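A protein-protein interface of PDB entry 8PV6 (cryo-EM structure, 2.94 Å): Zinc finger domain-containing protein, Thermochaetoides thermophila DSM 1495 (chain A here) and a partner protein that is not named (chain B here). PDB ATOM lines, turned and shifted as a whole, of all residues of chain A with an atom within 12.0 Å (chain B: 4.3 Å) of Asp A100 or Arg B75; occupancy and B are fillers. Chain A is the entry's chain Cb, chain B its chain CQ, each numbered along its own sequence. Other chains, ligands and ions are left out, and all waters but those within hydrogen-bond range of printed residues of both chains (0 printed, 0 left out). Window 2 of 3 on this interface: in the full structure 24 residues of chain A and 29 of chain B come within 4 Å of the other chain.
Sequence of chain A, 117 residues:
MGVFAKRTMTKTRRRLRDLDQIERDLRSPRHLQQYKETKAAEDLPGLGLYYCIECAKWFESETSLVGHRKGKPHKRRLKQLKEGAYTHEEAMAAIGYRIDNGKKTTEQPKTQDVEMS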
ATOM      1  N   GLU A  89      -8.176  25.406  -8.542  1.00  0.00           N
ATOM      2  CA  GLU A  89      -6.864  25.694  -9.112  1.00  0.00           C
ATOM      3  C   GLU A  89      -5.769  24.930  -8.380  1.00  0.00           C
ATOM      4  O   GLU A  89      -4.821  24.434  -9.001  1.00  0.00           O
ATOM      5  CB  GLU A  89      -6.588  27.199  -9.075  1.00  0.00           C
ATOM      6  CG  GLU A  89      -7.482  28.039  -9.982  1.00  0.00           C
ATOM      7  CD  GLU A  89      -8.830  28.367  -9.365  1.00  0.00           C
ATOM      8  OE1 GLU A  89      -9.060  27.996  -8.194  1.00  0.00           O
ATOM      9  OE2 GLU A  89      -9.663  28.991 -10.056  1.00  0.00           O
ATOM     10  N   MET A  92      -5.988  21.358  -9.605  1.00  0.00           N
ATOM     11  CA  MET A  92      -5.326  21.210 -10.899  1.00  0.00           C
ATOM     12  C   MET A  92      -3.808  21.255 -10.761  1.00  0.00           C
ATOM     13  O   MET A  92      -3.095  20.499 -11.432  1.00  0.00           O
ATOM     14  CB  MET A  92      -5.803  22.295 -11.858  1.00  0.00           C
ATOM     15  CG  MET A  92      -7.272  22.225 -12.203  1.00  0.00           C
ATOM     16  SD  MET A  92      -7.584  22.941 -13.822  1.00  0.00           S
ATOM     17  CE  MET A  92      -7.439  24.676 -13.413  1.00  0.00           C
ATOM     18  N   GLY A  96      -0.756  18.811 -11.852  1.00  0.00           N
ATOM     19  CA  GLY A  96      -0.022  19.466 -12.923  1.00  0.00           C
ATOM     20  C   GLY A  96      -0.841  19.707 -14.172  1.00  0.00           C
ATOM     21  O   GLY A  96      -0.360  19.455 -15.284  1.00  0.00           O
ATOM     22  N   TYR A  97      -2.066  20.193 -14.014  1.00  0.00           N
ATOM     23  CA  TYR A  97      -2.996  20.403 -15.110  1.00  0.00           C
ATOM     24  C   TYR A  97      -3.323  21.888 -15.216  1.00  0.00           C
ATOM     25  O   TYR A  97      -3.547  22.562 -14.208  1.00  0.00           O
ATOM     26  CB  TYR A  97      -4.272  19.587 -14.883  1.00  0.00           C
ATOM     27  CG  TYR A  97      -5.186  19.476 -16.076  1.00  0.00           C
ATOM     28  CD1 TYR A  97      -4.710  19.029 -17.300  1.00  0.00           C
ATOM     29  CD2 TYR A  97      -6.534  19.794 -15.973  1.00  0.00           C
ATOM     30  CE1 TYR A  97      -5.546  18.918 -18.391  1.00  0.00           C
ATOM     31  CE2 TYR A  97      -7.377  19.686 -17.058  1.00  0.00           C
ATOM     32  CZ  TYR A  97      -6.878  19.247 -18.264  1.00  0.00           C
ATOM     33  OH  TYR A  97      -7.713  19.136 -19.351  1.00  0.00           O
ATOM     34  N   ARG A  98      -3.332  22.401 -16.442  1.00  0.00           N
ATOM     35  CA  ARG A  98      -3.553  23.819 -16.685  1.00  0.00           C
ATOM     36  C   ARG A  98      -4.682  24.003 -17.691  1.00  0.00           C
ATOM     37  O   ARG A  98      -5.253  23.039 -18.204  1.00  0.00           O
ATOM     38  CB  ARG A  98      -2.276  24.504 -17.185  1.00  0.00           C
ATOM     39  CG  ARG A  98      -1.799  24.003 -18.531  1.00  0.00           C
ATOM     40  CD  ARG A  98      -0.544  24.726 -18.982  1.00  0.00           C
ATOM     41  NE  ARG A  98      -0.027  24.181 -20.231  1.00  0.00           N
ATOM     42  CZ  ARG A  98      -0.405  24.581 -21.437  1.00  0.00           C
ATOM     43  NH1 ARG A  98      -1.305  25.537 -21.598  1.00  0.00           N
ATOM     44  NH2 ARG A  98       0.133  24.008 -22.510  1.00  0.00           N
ATOM     45  N   ILE A  99      -5.006  25.265 -17.960  1.00  0.00           N
ATOM     46  CA  ILE A  99      -6.034  25.636 -18.926  1.00  0.00           C
ATOM     47  C   ILE A  99      -5.379  26.486 -20.004  1.00  0.00           C
ATOM     48  O   ILE A  99      -4.682  27.462 -19.696  1.00  0.00           O
ATOM     49  CB  ILE A  99      -7.199  26.392 -18.267  1.00  0.00           C
ATOM     50  CG1 ILE A  99      -7.913  25.506 -17.249  1.00  0.00           C
ATOM     51  CG2 ILE A  99      -8.196  26.856 -19.307  1.00  0.00           C
ATOM     52  CD1 ILE A  99      -8.896  26.262 -16.390  1.00  0.00           C
ATOM     53  N   ASP A 100      -5.597  26.117 -21.265  1.00  0.00           N
ATOM     54  CA  ASP A 100      -5.039  26.833 -22.405  1.00  0.00           C
ATOM     55  C   ASP A 100      -6.141  27.703 -23.002  1.00  0.00           C
ATOM     56  O   ASP A 100      -7.089  27.189 -23.603  1.00  0.00           O
ATOM     57  CB  ASP A 100      -4.485  25.849 -23.436  1.00  0.00           C
ATOM     58  CG  ASP A 100      -3.698  26.527 -24.549  1.00  0.00           C
ATOM     59  OD1 ASP A 100      -3.588  27.771 -24.563  1.00  0.00           O
ATOM     60  OD2 ASP A 100      -3.181  25.801 -25.424  1.00  0.00           O
ATOM     61  N   ASN A 101      -6.014  29.020 -22.835  1.00  0.00           N
ATOM     62  CA  ASN A 101      -6.939  29.984 -23.418  1.00  0.00           C
ATOM     63  C   ASN A 101      -6.360  30.666 -24.652  1.00  0.00           C
ATOM     64  O   ASN A 101      -6.940  31.637 -25.149  1.00  0.00           O
ATOM     65  CB  ASN A 101      -7.344  31.030 -22.379  1.00  0.00           C
ATOM     66  CG  ASN A 101      -8.146  30.439 -21.241  1.00  0.00           C
ATOM     67  OD1 ASN A 101      -8.735  29.370 -21.376  1.00  0.00           O
ATOM     68  ND2 ASN A 101      -8.169  31.132 -20.110  1.00  0.00           N
ATOM     69  N   GLY A 102      -5.231  30.183 -25.156  1.00  0.00           N
ATOM     70  CA  GLY A 102      -4.602  30.779 -26.318  1.00  0.00           C
ATOM     71  C   GLY A 102      -3.927  32.103 -26.016  1.00  0.00           C
ATOM     72  O   GLY A 102      -2.715  32.245 -26.177  1.00  0.00           O
ATOM     73  N   PHE B  71       2.282  19.565 -22.002  1.00  0.00           N
ATOM     74  CA  PHE B  71       1.617  18.979 -23.154  1.00  0.00           C
ATOM     75  C   PHE B  71       0.154  18.651 -22.892  1.00  0.00           C
ATOM     76  O   PHE B  71      -0.567  18.313 -23.835  1.00  0.00           O
ATOM     77  CB  PHE B  71       2.346  17.708 -23.603  1.00  0.00           C
ATOM     78  CG  PHE B  71       3.750  17.950 -24.069  1.00  0.00           C
ATOM     79  CD1 PHE B  71       3.999  18.392 -25.357  1.00  0.00           C
ATOM     80  CD2 PHE B  71       4.822  17.738 -23.219  1.00  0.00           C
ATOM     81  CE1 PHE B  71       5.289  18.615 -25.791  1.00  0.00           C
ATOM     82  CE2 PHE B  71       6.115  17.961 -23.647  1.00  0.00           C
ATOM     83  CZ  PHE B  71       6.348  18.400 -24.933  1.00  0.00           C
ATOM     84  N   ALA B  72      -0.298  18.745 -21.646  1.00  0.00           N
ATOM     85  CA  ALA B  72      -1.687  18.500 -21.287  1.00  0.00           C
ATOM     86  C   ALA B  72      -2.299  19.786 -20.752  1.00  0.00           C
ATOM     87  O   ALA B  72      -1.737  20.419 -19.852  1.00  0.00           O
ATOM     88  CB  ALA B  72      -1.798  17.386 -20.245  1.00  0.00           C
ATOM     89  N   ALA B  73      -3.447  20.166 -21.307  1.00  0.00           N
ATOM     90  CA  ALA B  73      -4.155  21.360 -20.873  1.00  0.00           C
ATOM     91  C   ALA B  73      -5.619  21.220 -21.254  1.00  0.00           C
ATOM     92  O   ALA B  73      -5.980  20.409 -22.108  1.00  0.00           O
ATOM     93  CB  ALA B  73      -3.560  22.628 -21.491  1.00  0.00           C
ATOM     94  N   ARG B  74      -6.460  22.023 -20.609  1.00  0.00           N
ATOM     95  CA  ARG B  74      -7.871  22.099 -20.978  1.00  0.00           C
ATOM     96  C   ARG B  74      -8.001  23.136 -22.085  1.00  0.00           C
ATOM     97  O   ARG B  74      -8.132  24.332 -21.820  1.00  0.00           O
ATOM     98  CB  ARG B  74      -8.733  22.454 -19.773  1.00  0.00           C
ATOM     99  CG  ARG B  74     -10.221  22.368 -20.049  1.00  0.00           C
ATOM    100  CD  ARG B  74     -11.034  22.667 -18.807  1.00  0.00           C
ATOM    101  NE  ARG B  74     -12.431  22.289 -18.974  1.00  0.00           N
ATOM    102  CZ  ARG B  74     -13.369  23.090 -19.460  1.00  0.00           C
ATOM    103  NH1 ARG B  74     -13.093  24.327 -19.838  1.00  0.00           N
ATOM    104  NH2 ARG B  74     -14.614  22.638 -19.570  1.00  0.00           N
ATOM    105  N   ARG B  75      -7.957  22.675 -23.331  1.00  0.00           N
ATOM    106  CA  ARG B  75      -7.954  23.569 -24.480  1.00  0.00           C
ATOM    107  C   ARG B  75      -9.343  24.162 -24.677  1.00  0.00           C
ATOM    108  O   ARG B  75     -10.296  23.440 -24.984  1.00  0.00           O
ATOM    109  CB  ARG B  75      -7.504  22.821 -25.731  1.00  0.00           C
ATOM    110  CG  ARG B  75      -6.383  21.829 -25.486  1.00  0.00           C
ATOM    111  CD  ARG B  75      -5.057  22.533 -25.273  1.00  0.00           C
ATOM    112  NE  ARG B  75      -3.958  21.585 -25.145  1.00  0.00           N
ATOM    113  CZ  ARG B  75      -2.685  21.927 -25.019  1.00  0.00           C
ATOM    114  NH1 ARG B  75      -2.309  23.195 -25.000  1.00  0.00           N
ATOM    115  NH2 ARG B  75      -1.765  20.974 -24.909  1.00  0.00           N
ATOM    116  N   ASN B  76      -9.453  25.478 -24.498  1.00  0.00           N
ATOM    117  CA  ASN B  76     -10.714  26.182 -24.663  1.00  0.00           C
ATOM    118  C   ASN B  76     -10.922  26.732 -26.064  1.00  0.00           C
ATOM    119  O   ASN B  76     -12.059  27.064 -26.416  1.00  0.00           O
ATOM    120  CB  ASN B  76     -10.814  27.328 -23.650  1.00  0.00           C
ATOM    121  CG  ASN B  76     -11.173  26.847 -22.264  1.00  0.00           C
ATOM    122  OD1 ASN B  76     -11.591  25.705 -22.081  1.00  0.00           O
ATOM    123  ND2 ASN B  76     -11.012  27.716 -21.279  1.00  0.00           N
ATOM    124  N   VAL B  77      -9.871  26.837 -26.867  1.00  0.00           N
ATOM    125  CA  VAL B  77      -9.969  27.257 -28.258  1.00  0.00           C
ATOM    126  C   VAL B  77      -9.863  26.001 -29.120  1.00  0.00           C
ATOM    127  O   VAL B  77      -8.775  25.417 -29.227  1.00  0.00           O
ATOM    128  CB  VAL B  77      -8.884  28.278 -28.622  1.00  0.00           C
ATOM    129  CG1 VAL B  77      -8.994  28.669 -30.083  1.00  0.00           C
ATOM    130  CG2 VAL B  77      -8.992  29.502 -27.732  1.00  0.00           C
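N of Gly A102 lies within hydrogen-bond range of OD1 of Asp A100, 3.0 Å away. The guanidinium group of Arg B74 is in hydrogen-bond range of the side-chain amide oxygen of Asn B76 (3.0 Å). The backbone carbonyl oxygen of Met A92 is in hydrogen-bond range of the backbone NH of Tyr A97, 2.8 Å away. The backbone carbonyl oxygen of Phe B71 lies within hydrogen-bond range of the guanidinium group of Arg B75 (3.1 Å).
Of the 9 printed residues of chain A, 5 touch a printed residue of chain B. Hydrophobic or aromatic side chains of chain A within 4 Å of the printed part of chain B: Tyr A97 and Ile A99. Of the 7 printed residues of chain B, 6 touch a printed residue of chain A. Printed residues of chain B that touch a printed residue of chain A: Ala B72, Ala B73, Arg B74, Arg B75, Asn B76 and Val B77.
Printed residues of chain B within 4 Å of Tyr A97: Ala B73 (3.5 Å) and Arg B74 (3.4 Å). Of the printed residues of chain B, Arg A98 touches Ala B72 (3.8 Å), Ala B73 (3.3 Å), Arg B74 (2.9 Å) and Arg B75 (3.6 Å). Printed residues of chain B within 4 Å of Ile A99: Arg B74 and Asn B76. Printed residues of chain B within 4 Å of Asp A100: Ala B73 (3.9 Å), Arg B74 (3.1 Å), Arg B75 (2.8 Å) and Asn B76 (3.1 Å). Printed residues of chain B within 4 Å of Asn A101: Asn B76 and Val B77. Printed residues of chain A within 4 Å of Ala B72: Arg A98. Arg B74 touches four residues of chain A. Arg B75 touches just these residues of chain A: Arg A98 and Asp A100. Printed residues of chain A within 4 Å of Val B77: Asn A101. The nearest printed residue of chain B that does not touch Asp A100 is Val B77 (4.3 Å).
The backbone carbonyl oxygen (O) of Arg A98 lies within hydrogen-bond range of the backbone NH (N) of Arg B74, 2.9 Å away. OH of Tyr A97 sits close to N of Arg B74, 3.4 Å away. The backbone carbonyl oxygen (O) of Ala B73 is in hydrogen-bond range of the side-chain hydroxyl (OH) of Tyr A97. ND2 of Asn B76 lies within hydrogen-bond range of OD1 of Asn A101. The backbone carbonyl oxygen (O) of Asp A100 sits at hydrogen-bond distance from the backbone NH (N) of Asn B76 (3.1 Å). The guanidinium group (NH1) of Arg B75 lies within salt-bridge range of the side-chain carboxylate (OD2) of Asp A100. The backbone carbonyl oxygen (O) of Arg B74 is in hydrogen-bond range of the backbone NH (N) of Asp A100, at 3.1 Å.
Ala B72 touches Arg A98 (O to CG, 3.8 Å). Arg A98 touches Ala B73 (O to CA, 3.3 Å). Arg B75 touches Arg A98. Arg B74 touches Ile A99 (O to CG2, 3.6 Å). Asn B76 touches Ile A99. CB of Asp A100 touches CB of Ala B73, at 3.9 Å. Asn A101 touches Val B77 (O to CG2, 3.9 Å).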
